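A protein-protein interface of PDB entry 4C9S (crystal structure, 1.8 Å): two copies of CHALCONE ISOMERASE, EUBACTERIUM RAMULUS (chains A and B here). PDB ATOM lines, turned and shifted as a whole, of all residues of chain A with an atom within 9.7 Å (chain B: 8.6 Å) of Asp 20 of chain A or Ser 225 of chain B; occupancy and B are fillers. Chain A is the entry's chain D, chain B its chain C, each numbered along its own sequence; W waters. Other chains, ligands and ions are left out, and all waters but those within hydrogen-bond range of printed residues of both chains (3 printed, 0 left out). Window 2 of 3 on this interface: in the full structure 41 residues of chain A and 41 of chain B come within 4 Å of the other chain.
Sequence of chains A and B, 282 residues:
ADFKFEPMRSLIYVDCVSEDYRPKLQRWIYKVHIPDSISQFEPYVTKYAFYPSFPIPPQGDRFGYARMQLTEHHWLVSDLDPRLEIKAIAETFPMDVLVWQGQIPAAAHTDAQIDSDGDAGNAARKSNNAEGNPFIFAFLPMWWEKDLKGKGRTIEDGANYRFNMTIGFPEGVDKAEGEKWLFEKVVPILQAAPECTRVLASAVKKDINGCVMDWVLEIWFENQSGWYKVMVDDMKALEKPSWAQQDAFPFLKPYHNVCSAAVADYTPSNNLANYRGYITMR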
ATOM      1  N   CYS A  16       0.552  -3.257  -3.414  1.00  0.00           N
ATOM      2  CA  CYS A  16      -0.367  -3.550  -4.467  1.00  0.00           C
ATOM      3  C   CYS A  16      -1.632  -4.040  -3.728  1.00  0.00           C
ATOM      4  O   CYS A  16      -1.622  -5.115  -3.151  1.00  0.00           O
ATOM      5  CB  CYS A  16       0.189  -4.602  -5.418  1.00  0.00           C
ATOM      6  SG  CYS A  16      -0.972  -4.884  -6.812  1.00  0.00           S
ATOM      7  N   VAL A  17      -2.652  -3.195  -3.669  1.00  0.00           N
ATOM      8  CA  VAL A  17      -3.719  -3.419  -2.695  1.00  0.00           C
ATOM      9  C   VAL A  17      -4.787  -4.368  -3.134  1.00  0.00           C
ATOM     10  O   VAL A  17      -5.555  -4.837  -2.298  1.00  0.00           O
ATOM     11  CB  VAL A  17      -4.394  -2.117  -2.250  1.00  0.00           C
ATOM     12  CG1 VAL A  17      -3.395  -1.263  -1.577  1.00  0.00           C
ATOM     13  CG2 VAL A  17      -5.057  -1.370  -3.375  1.00  0.00           C
ATOM     14  N   SER A  18      -4.800  -4.740  -4.398  1.00  0.00           N
ATOM     15  CA  SER A  18      -5.676  -5.784  -4.888  1.00  0.00           C
ATOM     16  C   SER A  18      -4.934  -6.540  -5.964  1.00  0.00           C
ATOM     17  O   SER A  18      -4.168  -5.923  -6.772  1.00  0.00           O
ATOM     18  CB  SER A  18      -6.918  -5.123  -5.509  1.00  0.00           C
ATOM     19  OG  SER A  18      -7.672  -6.073  -6.239  1.00  0.00           O
ATOM     20  N   GLU A  19      -5.132  -7.850  -6.016  1.00  0.00           N
ATOM     21  CA  GLU A  19      -4.510  -8.617  -7.107  1.00  0.00           C
ATOM     22  C   GLU A  19      -4.959  -8.157  -8.471  1.00  0.00           C
ATOM     23  O   GLU A  19      -4.211  -8.239  -9.432  1.00  0.00           O
ATOM     24  CB  GLU A  19      -4.730 -10.120  -6.892  1.00  0.00           C
ATOM     25  CG  GLU A  19      -3.931 -10.606  -5.680  1.00  0.00           C
ATOM     26  CD  GLU A  19      -2.463 -10.311  -5.837  1.00  0.00           C
ATOM     27  OE1 GLU A  19      -1.917 -10.571  -6.944  1.00  0.00           O
ATOM     28  OE2 GLU A  19      -1.809  -9.747  -4.890  1.00  0.00           O
ATOM     29  N   ASP A  20      -6.157  -7.601  -8.580  1.00  0.00           N
ATOM     30  CA  ASP A  20      -6.597  -7.097  -9.863  1.00  0.00           C
ATOM     31  C   ASP A  20      -5.799  -5.931 -10.414  1.00  0.00           C
ATOM     32  O   ASP A  20      -5.862  -5.669 -11.597  1.00  0.00           O
ATOM     33  CB  ASP A  20      -8.058  -6.755  -9.862  1.00  0.00           C
ATOM     34  CG  ASP A  20      -8.957  -8.013  -9.815  1.00  0.00           C
ATOM     35  OD1 ASP A  20      -8.520  -9.129 -10.187  1.00  0.00           O
ATOM     36  OD2 ASP A  20     -10.104  -7.863  -9.405  1.00  0.00           O
ATOM     37  N   TYR A  21      -5.029  -5.275  -9.554  1.00  0.00           N
ATOM     38  CA  TYR A  21      -4.214  -4.152 -10.015  1.00  0.00           C
ATOM     39  C   TYR A  21      -2.830  -4.589 -10.393  1.00  0.00           C
ATOM     40  O   TYR A  21      -2.050  -3.789 -10.936  1.00  0.00           O
ATOM     41  CB  TYR A  21      -4.118  -3.150  -8.900  1.00  0.00           C
ATOM     42  CG  TYR A  21      -5.408  -2.494  -8.437  1.00  0.00           C
ATOM     43  CD1 TYR A  21      -6.464  -2.243  -9.304  1.00  0.00           C
ATOM     44  CD2 TYR A  21      -5.536  -2.039  -7.142  1.00  0.00           C
ATOM     45  CE1 TYR A  21      -7.610  -1.594  -8.876  1.00  0.00           C
ATOM     46  CE2 TYR A  21      -6.682  -1.364  -6.702  1.00  0.00           C
ATOM     47  CZ  TYR A  21      -7.715  -1.170  -7.578  1.00  0.00           C
ATOM     48  OH  TYR A  21      -8.838  -0.489  -7.159  1.00  0.00           O
ATOM     49  N   ARG A  22      -2.454  -5.819 -10.039  1.00  0.00           N
ATOM     50  CA  ARG A  22      -1.059  -6.222 -10.198  1.00  0.00           C
ATOM     51  C   ARG A  22      -0.544  -6.094 -11.629  1.00  0.00           C
ATOM     52  O   ARG A  22       0.549  -5.549 -11.839  1.00  0.00           O
ATOM     53  CB  ARG A  22      -0.830  -7.624  -9.610  1.00  0.00           C
ATOM     54  CG  ARG A  22       0.609  -8.116  -9.718  1.00  0.00           C
ATOM     55  CD  ARG A  22       0.813  -9.461  -8.992  1.00  0.00           C
ATOM     56  NE  ARG A  22       0.472  -9.394  -7.592  1.00  0.00           N
ATOM     57  CZ  ARG A  22       1.340  -8.981  -6.653  1.00  0.00           C
ATOM     58  NH1 ARG A  22       2.536  -8.588  -6.995  1.00  0.00           N
ATOM     59  NH2 ARG A  22       1.006  -8.929  -5.373  1.00  0.00           N
ATOM     60  N   PRO A  23      -1.316  -6.569 -12.642  1.00  0.00           N
ATOM     61  CA  PRO A  23      -0.787  -6.420 -13.982  1.00  0.00           C
ATOM     62  C   PRO A  23      -0.547  -4.959 -14.389  1.00  0.00           C
ATOM     63  O   PRO A  23       0.464  -4.636 -15.047  1.00  0.00           O
ATOM     64  CB  PRO A  23      -1.834  -7.091 -14.868  1.00  0.00           C
ATOM     65  CG  PRO A  23      -2.459  -8.117 -13.986  1.00  0.00           C
ATOM     66  CD  PRO A  23      -2.536  -7.402 -12.634  1.00  0.00           C
ATOM     67  N   LYS A  24      -1.485  -4.081 -14.048  1.00  0.00           N
ATOM     68  CA  LYS A  24      -1.341  -2.682 -14.443  1.00  0.00           C
ATOM     69  C   LYS A  24      -0.165  -2.010 -13.708  1.00  0.00           C
ATOM     70  O   LYS A  24       0.608  -1.235 -14.304  1.00  0.00           O
ATOM     71  CB  LYS A  24      -2.646  -1.939 -14.130  1.00  0.00           C
ATOM     72  CG  LYS A  24      -3.742  -2.287 -15.129  1.00  0.00           C
ATOM     73  CD  LYS A  24      -5.035  -1.767 -14.608  1.00  0.00           C
ATOM     74  CE  LYS A  24      -6.113  -1.825 -15.645  1.00  0.00           C
ATOM     75  NZ  LYS A  24      -6.520  -3.241 -15.924  1.00  0.00           N
ATOM     76  N   LEU A  25      -0.061  -2.261 -12.420  1.00  0.00           N
ATOM     77  CA  LEU A  25       1.018  -1.661 -11.598  1.00  0.00           C
ATOM     78  C   LEU A  25       2.389  -2.130 -12.060  1.00  0.00           C
ATOM     79  O   LEU A  25       3.297  -1.345 -12.292  1.00  0.00           O
ATOM     80  CB  LEU A  25       0.839  -1.935 -10.138  1.00  0.00           C
ATOM     81  CG  LEU A  25       1.902  -1.378  -9.163  1.00  0.00           C
ATOM     82  CD1 LEU A  25       2.077   0.120  -9.285  1.00  0.00           C
ATOM     83  CD2 LEU A  25       1.534  -1.712  -7.735  1.00  0.00           C
ATOM     84  N   GLN A  26       2.511  -3.429 -12.258  1.00  0.00           N
ATOM     85  CA  GLN A  26       3.768  -3.997 -12.726  1.00  0.00           C
ATOM     86  C   GLN A  26       4.156  -3.461 -14.090  1.00  0.00           C
ATOM     87  O   GLN A  26       5.335  -3.149 -14.328  1.00  0.00           O
ATOM     88  CB  GLN A  26       3.664  -5.523 -12.703  1.00  0.00           C
ATOM     89  CG  GLN A  26       4.969  -6.254 -12.778  1.00  0.00           C
ATOM     90  CD  GLN A  26       4.770  -7.717 -12.291  1.00  0.00           C
ATOM     91  OE1 GLN A  26       4.224  -7.962 -11.204  1.00  0.00           O
ATOM     92  NE2 GLN A  26       5.136  -8.648 -13.114  1.00  0.00           N
ATOM     93  N   ARG A  67       2.994  -5.496  -0.928  1.00  0.00           N
ATOM     94  CA  ARG A  67       2.690  -6.632  -1.753  1.00  0.00           C
ATOM     95  C   ARG A  67       3.308  -6.590  -3.179  1.00  0.00           C
ATOM     96  O   ARG A  67       3.159  -7.569  -3.936  1.00  0.00           O
ATOM     97  CB  ARG A  67       1.166  -6.899  -1.773  1.00  0.00           C
ATOM     98  CG  ARG A  67       0.645  -7.465  -0.473  1.00  0.00           C
ATOM     99  CD  ARG A  67      -0.866  -7.351  -0.258  1.00  0.00           C
ATOM    100  NE  ARG A  67      -1.198  -5.996   0.085  1.00  0.00           N
ATOM    101  CZ  ARG A  67      -2.401  -5.588   0.413  1.00  0.00           C
ATOM    102  NH1 ARG A  67      -3.399  -6.470   0.478  1.00  0.00           N
ATOM    103  NH2 ARG A  67      -2.611  -4.319   0.688  1.00  0.00           N
ATOM    104  N   MET A  68       3.944  -5.479  -3.579  1.00  0.00           N
ATOM    105  CA  MET A  68       4.618  -5.418  -4.849  1.00  0.00           C
ATOM    106  C   MET A  68       6.108  -5.597  -4.677  1.00  0.00           C
ATOM    107  O   MET A  68       6.692  -6.619  -5.111  1.00  0.00           O
ATOM    108  CB  MET A  68       4.284  -4.112  -5.579  1.00  0.00           C
ATOM    109  CG  MET A  68       4.908  -4.000  -6.965  1.00  0.00           C
ATOM    110  SD  MET A  68       4.512  -5.295  -8.156  1.00  0.00           S
ATOM    111  CE  MET A  68       2.879  -5.004  -8.366  1.00  0.00           C
ATOM    112  N   VAL A  99      -3.946   4.678  -6.735  1.00  0.00           N
ATOM    113  CA  VAL A  99      -4.974   3.682  -6.358  1.00  0.00           C
ATOM    114  C   VAL A  99      -4.345   2.277  -6.246  1.00  0.00           C
ATOM    115  O   VAL A  99      -4.568   1.570  -5.285  1.00  0.00           O
ATOM    116  CB  VAL A  99      -6.083   3.663  -7.403  1.00  0.00           C
ATOM    117  CG1 VAL A  99      -7.136   2.640  -7.071  1.00  0.00           C
ATOM    118  CG2 VAL A  99      -6.694   5.075  -7.505  1.00  0.00           C
ATOM    119  N   TRP A 100      -3.503   1.897  -7.218  1.00  0.00           N
ATOM    120  CA  TRP A 100      -2.974   0.545  -7.234  1.00  0.00           C
ATOM    121  C   TRP A 100      -2.075   0.294  -6.024  1.00  0.00           C
ATOM    122  O   TRP A 100      -2.111  -0.778  -5.440  1.00  0.00           O
ATOM    123  CB  TRP A 100      -2.246   0.243  -8.539  1.00  0.00           C
ATOM    124  CG  TRP A 100      -3.021   0.495  -9.799  1.00  0.00           C
ATOM    125  CD1 TRP A 100      -4.365   0.401  -9.995  1.00  0.00           C
ATOM    126  CD2 TRP A 100      -2.483   0.921 -11.079  1.00  0.00           C
ATOM    127  NE1 TRP A 100      -4.696   0.711 -11.262  1.00  0.00           N
ATOM    128  CE2 TRP A 100      -3.596   1.018 -11.973  1.00  0.00           C
ATOM    129  CE3 TRP A 100      -1.217   1.179 -11.566  1.00  0.00           C
ATOM    130  CZ2 TRP A 100      -3.452   1.443 -13.255  1.00  0.00           C
ATOM    131  CZ3 TRP A 100      -1.075   1.589 -12.853  1.00  0.00           C
ATOM    132  CH2 TRP A 100      -2.159   1.726 -13.694  1.00  0.00           C
ATOM    133  N   PRO B  57      -4.237 -17.981  -8.094  1.00  0.00           N
ATOM    134  CA  PRO B  57      -5.590 -17.473  -7.942  1.00  0.00           C
ATOM    135  C   PRO B  57      -6.477 -18.484  -7.202  1.00  0.00           C
ATOM    136  O   PRO B  57      -6.078 -19.622  -7.010  1.00  0.00           O
ATOM    137  CB  PRO B  57      -6.059 -17.286  -9.380  1.00  0.00           C
ATOM    138  CG  PRO B  57      -5.319 -18.327 -10.163  1.00  0.00           C
ATOM    139  CD  PRO B  57      -3.976 -18.509  -9.444  1.00  0.00           C
ATOM    140  N   PRO B  58      -7.650 -18.049  -6.742  1.00  0.00           N
ATOM    141  CA  PRO B  58      -8.588 -18.990  -6.111  1.00  0.00           C
ATOM    142  C   PRO B  58      -8.938 -20.144  -7.028  1.00  0.00           C
ATOM    143  O   PRO B  58      -9.251 -19.923  -8.197  1.00  0.00           O
ATOM    144  CB  PRO B  58      -9.845 -18.107  -5.836  1.00  0.00           C
ATOM    145  CG  PRO B  58      -9.319 -16.736  -5.780  1.00  0.00           C
ATOM    146  CD  PRO B  58      -8.196 -16.686  -6.782  1.00  0.00           C
ATOM    147  N   ALA B 159      -2.119  -3.979 -20.174  1.00  0.00           N
ATOM    148  CA  ALA B 159      -1.465  -5.111 -19.449  1.00  0.00           C
ATOM    149  C   ALA B 159      -2.276  -6.376 -19.496  1.00  0.00           C
ATOM    150  O   ALA B 159      -3.493  -6.332 -19.229  1.00  0.00           O
ATOM    151  CB  ALA B 159      -1.291  -4.719 -18.010  1.00  0.00           C
ATOM    152  N   TYR B 161      -3.081 -10.348 -18.163  1.00  0.00           N
ATOM    153  CA  TYR B 161      -2.946 -11.473 -17.208  1.00  0.00           C
ATOM    154  C   TYR B 161      -2.943 -12.721 -18.089  1.00  0.00           C
ATOM    155  O   TYR B 161      -4.012 -13.141 -18.608  1.00  0.00           O
ATOM    156  CB  TYR B 161      -4.158 -11.432 -16.284  1.00  0.00           C
ATOM    157  CG  TYR B 161      -4.179 -12.436 -15.139  1.00  0.00           C
ATOM    158  CD1 TYR B 161      -3.563 -12.145 -13.910  1.00  0.00           C
ATOM    159  CD2 TYR B 161      -4.776 -13.654 -15.303  1.00  0.00           C
ATOM    160  CE1 TYR B 161      -3.612 -13.058 -12.842  1.00  0.00           C
ATOM    161  CE2 TYR B 161      -4.853 -14.582 -14.271  1.00  0.00           C
ATOM    162  CZ  TYR B 161      -4.249 -14.275 -13.037  1.00  0.00           C
ATOM    163  OH  TYR B 161      -4.340 -15.199 -12.019  1.00  0.00           O
ATOM    164  N   GLU B 195     -14.431 -10.731 -20.940  1.00  0.00           N
ATOM    165  CA  GLU B 195     -13.250 -10.616 -20.061  1.00  0.00           C
ATOM    166  C   GLU B 195     -11.997 -11.234 -20.692  1.00  0.00           C
ATOM    167  O   GLU B 195     -10.887 -11.029 -20.182  1.00  0.00           O
ATOM    168  CB  GLU B 195     -13.541 -11.366 -18.740  1.00  0.00           C
ATOM    169  CG  GLU B 195     -14.719 -10.761 -17.930  1.00  0.00           C
ATOM    170  CD  GLU B 195     -16.131 -11.203 -18.388  1.00  0.00           C
ATOM    171  OE1 GLU B 195     -16.293 -12.088 -19.244  1.00  0.00           O
ATOM    172  OE2 GLU B 195     -17.117 -10.647 -17.816  1.00  0.00           O
ATOM    173  N   PHE B 221      -6.592 -12.422 -19.834  1.00  0.00           N
ATOM    174  CA  PHE B 221      -7.605 -11.679 -19.116  1.00  0.00           C
ATOM    175  C   PHE B 221      -7.009 -10.343 -18.701  1.00  0.00           C
ATOM    176  O   PHE B 221      -5.822 -10.069 -18.973  1.00  0.00           O
ATOM    177  CB  PHE B 221      -8.053 -12.479 -17.875  1.00  0.00           C
ATOM    178  CG  PHE B 221      -8.594 -13.804 -18.220  1.00  0.00           C
ATOM    179  CD1 PHE B 221      -9.918 -13.950 -18.613  1.00  0.00           C
ATOM    180  CD2 PHE B 221      -7.762 -14.919 -18.254  1.00  0.00           C
ATOM    181  CE1 PHE B 221     -10.402 -15.212 -18.952  1.00  0.00           C
ATOM    182  CE2 PHE B 221      -8.230 -16.163 -18.665  1.00  0.00           C
ATOM    183  CZ  PHE B 221      -9.576 -16.297 -18.989  1.00  0.00           C
ATOM    184  N   GLU B 222      -7.840  -9.463 -18.155  1.00  0.00           N
ATOM    185  CA  GLU B 222      -7.343  -8.256 -17.553  1.00  0.00           C
ATOM    186  C   GLU B 222      -6.678  -8.485 -16.226  1.00  0.00           C
ATOM    187  O   GLU B 222      -5.732  -7.752 -15.827  1.00  0.00           O
ATOM    188  CB  GLU B 222      -8.528  -7.299 -17.409  1.00  0.00           C
ATOM    189  CG  GLU B 222      -8.156  -5.907 -16.951  1.00  0.00           C
ATOM    190  CD  GLU B 222      -9.359  -4.948 -16.986  1.00  0.00           C
ATOM    191  OE1 GLU B 222     -10.542  -5.406 -17.114  1.00  0.00           O
ATOM    192  OE2 GLU B 222      -9.079  -3.728 -16.857  1.00  0.00           O
ATOM    193  N   ASN B 223      -7.205  -9.469 -15.498  1.00  0.00           N
ATOM    194  CA  ASN B 223      -6.858  -9.653 -14.113  1.00  0.00           C
ATOM    195  C   ASN B 223      -7.399 -10.970 -13.611  1.00  0.00           C
ATOM    196  O   ASN B 223      -8.126 -11.651 -14.313  1.00  0.00           O
ATOM    197  CB  ASN B 223      -7.387  -8.509 -13.244  1.00  0.00           C
ATOM    198  CG  ASN B 223      -8.858  -8.205 -13.494  1.00  0.00           C
ATOM    199  OD1 ASN B 223      -9.701  -9.084 -13.557  1.00  0.00           O
ATOM    200  ND2 ASN B 223      -9.190  -6.916 -13.546  1.00  0.00           N
ATOM    201  N   GLN B 224      -6.983 -11.301 -12.410  1.00  0.00           N
ATOM    202  CA  GLN B 224      -7.363 -12.511 -11.739  1.00  0.00           C
ATOM    203  C   GLN B 224      -8.911 -12.649 -11.627  1.00  0.00           C
ATOM    204  O   GLN B 224      -9.429 -13.762 -11.763  1.00  0.00           O
ATOM    205  CB  GLN B 224      -6.729 -12.535 -10.320  1.00  0.00           C
ATOM    206  CG  GLN B 224      -7.278 -13.591  -9.410  1.00  0.00           C
ATOM    207  CD  GLN B 224      -6.638 -13.465  -8.033  1.00  0.00           C
ATOM    208  OE1 GLN B 224      -5.487 -13.822  -7.850  1.00  0.00           O
ATOM    209  NE2 GLN B 224      -7.382 -12.924  -7.100  1.00  0.00           N
ATOM    210  N   SER B 225      -9.641 -11.560 -11.361  1.00  0.00           N
ATOM    211  CA  SER B 225     -11.130 -11.654 -11.259  1.00  0.00           C
ATOM    212  C   SER B 225     -11.739 -12.123 -12.571  1.00  0.00           C
ATOM    213  O   SER B 225     -12.650 -12.943 -12.595  1.00  0.00           O
ATOM    214  CB  SER B 225     -11.765 -10.315 -10.854  1.00  0.00           C
ATOM    215  OG  SER B 225     -11.463 -10.125  -9.502  1.00  0.00           O
ATOM    216  N   GLY B 226     -11.200 -11.613 -13.670  1.00  0.00           N
ATOM    217  CA  GLY B 226     -11.637 -12.014 -15.006  1.00  0.00           C
ATOM    218  C   GLY B 226     -11.346 -13.481 -15.246  1.00  0.00           C
ATOM    219  O   GLY B 226     -12.183 -14.226 -15.783  1.00  0.00           O
ATOM    220  N   TRP B 227     -10.153 -13.923 -14.866  1.00  0.00           N
ATOM    221  CA  TRP B 227      -9.777 -15.318 -14.996  1.00  0.00           C
ATOM    222  C   TRP B 227     -10.789 -16.212 -14.248  1.00  0.00           C
ATOM    223  O   TRP B 227     -11.260 -17.236 -14.784  1.00  0.00           O
ATOM    224  CB  TRP B 227      -8.338 -15.535 -14.507  1.00  0.00           C
ATOM    225  CG  TRP B 227      -7.945 -16.950 -14.465  1.00  0.00           C
ATOM    226  CD1 TRP B 227      -7.362 -17.696 -15.461  1.00  0.00           C
ATOM    227  CD2 TRP B 227      -8.207 -17.886 -13.374  1.00  0.00           C
ATOM    228  NE1 TRP B 227      -7.236 -18.991 -15.063  1.00  0.00           N
ATOM    229  CE2 TRP B 227      -7.731 -19.164 -13.813  1.00  0.00           C
ATOM    230  CE3 TRP B 227      -8.730 -17.756 -12.093  1.00  0.00           C
ATOM    231  CZ2 TRP B 227      -7.806 -20.297 -13.011  1.00  0.00           C
ATOM    232  CZ3 TRP B 227      -8.846 -18.896 -11.299  1.00  0.00           C
ATOM    233  CH2 TRP B 227      -8.385 -20.139 -11.746  1.00  0.00           C
ATOM    234  N   TYR B 228     -11.112 -15.839 -13.031  1.00  0.00           N
ATOM    235  CA  TYR B 228     -11.993 -16.651 -12.197  1.00  0.00           C
ATOM    236  C   TYR B 228     -13.402 -16.665 -12.803  1.00  0.00           C
ATOM    237  O   TYR B 228     -14.047 -17.714 -12.914  1.00  0.00           O
ATOM    238  CB  TYR B 228     -12.013 -16.087 -10.789  1.00  0.00           C
ATOM    239  CG  TYR B 228     -12.843 -16.930  -9.829  1.00  0.00           C
ATOM    240  CD1 TYR B 228     -14.233 -16.787  -9.759  1.00  0.00           C
ATOM    241  CD2 TYR B 228     -12.240 -17.936  -9.065  1.00  0.00           C
ATOM    242  CE1 TYR B 228     -14.977 -17.579  -8.909  1.00  0.00           C
ATOM    243  CE2 TYR B 228     -12.992 -18.695  -8.173  1.00  0.00           C
ATOM    244  CZ  TYR B 228     -14.351 -18.506  -8.124  1.00  0.00           C
ATOM    245  OH  TYR B 228     -15.140 -19.275  -7.272  1.00  0.00           O
ATOM    246  N   LYS B 229     -13.908 -15.494 -13.180  1.00  0.00           N
ATOM    247  CA  LYS B 229     -15.253 -15.413 -13.741  1.00  0.00           C
ATOM    248  C   LYS B 229     -15.385 -16.381 -14.897  1.00  0.00           C
ATOM    249  O   LYS B 229     -16.377 -17.125 -15.022  1.00  0.00           O
ATOM    250  CB  LYS B 229     -15.525 -13.983 -14.189  1.00  0.00           C
ATOM    251  CG  LYS B 229     -16.934 -13.755 -14.793  1.00  0.00           C
ATOM    252  CD  LYS B 229     -16.942 -13.948 -16.301  1.00  0.00           C
ATOM    253  CE  LYS B 229     -18.324 -13.618 -16.935  1.00  0.00           C
ATOM    254  NZ  LYS B 229     -18.327 -13.862 -18.436  1.00  0.00           N
ATOM    255  N   VAL B 230     -14.414 -16.363 -15.796  1.00  0.00           N
ATOM    256  CA  VAL B 230     -14.449 -17.215 -16.989  1.00  0.00           C
ATOM    257  C   VAL B 230     -14.051 -18.682 -16.724  1.00  0.00           C
ATOM    258  O   VAL B 230     -14.804 -19.606 -17.073  1.00  0.00           O
ATOM    259  CB  VAL B 230     -13.588 -16.657 -18.096  1.00  0.00           C
ATOM    260  CG1 VAL B 230     -13.624 -17.547 -19.315  1.00  0.00           C
ATOM    261  CG2 VAL B 230     -14.047 -15.264 -18.441  1.00  0.00           C
ATOM    262  N   MET B 231     -12.914 -18.934 -16.052  1.00  0.00           N
ATOM    263  CA  MET B 231     -12.378 -20.278 -15.973  1.00  0.00           C
ATOM    264  C   MET B 231     -13.023 -21.133 -14.873  1.00  0.00           C
ATOM    265  O   MET B 231     -12.901 -22.333 -14.924  1.00  0.00           O
ATOM    266  CB  MET B 231     -10.861 -20.261 -15.791  1.00  0.00           C
ATOM    267  CG  MET B 231     -10.157 -19.464 -16.914  1.00  0.00           C
ATOM    268  SD  MET B 231     -10.302 -20.222 -18.543  1.00  0.00           S
ATOM    269  CE  MET B 231      -9.228 -21.602 -18.352  1.00  0.00           C
ATOM    270  N   VAL B 232     -13.656 -20.497 -13.904  1.00  0.00           N
ATOM    271  CA  VAL B 232     -14.387 -21.180 -12.862  1.00  0.00           C
ATOM    272  C   VAL B 232     -15.901 -20.979 -13.148  1.00  0.00           C
ATOM    273  O   VAL B 232     -16.593 -21.941 -13.444  1.00  0.00           O
ATOM    274  CB  VAL B 232     -13.985 -20.702 -11.481  1.00  0.00           C
ATOM    275  CG1 VAL B 232     -14.805 -21.399 -10.377  1.00  0.00           C
ATOM    276  CG2 VAL B 232     -12.519 -21.010 -11.298  1.00  0.00           C
ATOM    277  N   ASP B 233     -16.402 -19.766 -13.112  1.00  0.00           N
ATOM    278  CA  ASP B 233     -17.870 -19.598 -13.146  1.00  0.00           C
ATOM    279  C   ASP B 233     -18.465 -19.925 -14.520  1.00  0.00           C
ATOM    280  O   ASP B 233     -19.417 -20.712 -14.579  1.00  0.00           O
ATOM    281  CB  ASP B 233     -18.339 -18.236 -12.665  1.00  0.00           C
ATOM    282  CG  ASP B 233     -18.205 -18.038 -11.183  1.00  0.00           C
ATOM    283  OD1 ASP B 233     -18.117 -18.991 -10.399  1.00  0.00           O
ATOM    284  OD2 ASP B 233     -18.118 -16.860 -10.782  1.00  0.00           O
HETATM  285  O   HOH W   1      -4.782  -5.395 -16.553  1.00  0.00           O
HETATM  286  O   HOH W   2      -7.483  -4.614 -13.422  1.00  0.00           O
HETATM  287  O   HOH W   3      -4.652  -9.852 -11.566  1.00  0.00           O
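Of the printed residues of chain B, Glu 19 of chain A touches Gln 224. Printed residues of chain B within 4 Å of Lys 24 of chain A: Glu 222. Met 68 of chain A touches none of the printed residues of chain B. Asn 223 of chain B touches just one residue of chain A: Asp 20 (3.3 Å). Of the printed residues of chain A, Gln 224 of chain B touches Glu 19 (3.9 Å) and Asp 20 (3.5 Å). Printed residues of chain A within 4 Å of Ser 225 of chain B: Asp 20 (2.6 Å). No residue of chain A comes within 4 Å of Gly 226 of chain B. Val 232 of chain B touches none of the printed residues of chain A. The nearest residue of chain A that does not touch Ser 225 of chain B is Ser 18 of chain A (6.4 Å).
Water W1 lies within hydrogen-bond range of the backbone carbonyl oxygen of Glu 222 of chain B (2.6 Å), the side-chain amino group of Lys 24 of chain A (2.8 Å) and the backbone carbonyl oxygen of Ala 159 of chain B (3.1 Å). Water W2 lies within hydrogen-bond range of O of Asp 20 of chain A (2.7 Å), ND2 of Asn 223 of chain B (2.9 Å) and NZ of Lys 24 of chain A (3.0 Å). Water W3 bridges O of Glu 19 of chain A (2.7 Å) and N of Gln 224 of chain B (2.9 Å).
The side-chain amino group (NZ) of Lys 24 of chain A lies within salt-bridge range of the side-chain carboxylate (OE2) of Glu 222 of chain B, at 2.8 Å. OD1 of Asp 20 of chain A is in hydrogen-bond range of N of Gln 224 of chain B (3.5 Å). The side-chain carboxylate (OD2) of Asp 20 of chain A sits at hydrogen-bond distance from the side-chain hydroxyl (OG) of Ser 225 of chain B.
OD1 of Asn 223 of chain B sits close to N of Ser 225 of chain B (3.3 Å). The side-chain amide oxygen (OD1) of Asn 223 of chain B lies within hydrogen-bond range of the backbone NH (N) of Gly 226 of chain B (2.9 Å). OG of Ser 18 of chain A lies close to N of Asp 20 of chain A, 3.2 Å away. The guanidinium group of Arg 22 of chain A lies within salt-bridge range of the side-chain carboxylate of Glu 19 of chain A (2.7 Å).
Of the 15 printed residues of chain A, 4 touch a printed residue of chain B. Hydrophobic or aromatic side chains of chain A within 4 Å of the printed part of chain B: Pro 23. Of the 18 printed residues of chain B, 5 touch a printed residue of chain A.
Among the printed residues, merely in contact across the chains: Glu 19 of chain A with Gln 224 of chain B (3.9 Å), Asp 20 of chain A with Asn 223 of chain B (3.3 Å), Pro 23 of chain A with Ala 159 of chain B (3.4 Å) and Pro 23 of chain A with Glu 222 of chain B (3.8 Å).
No position is printed for both chains. Of the 7 pairs that touch across the chains among the printed residues, none has its exchanged pair printed and touching as well.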
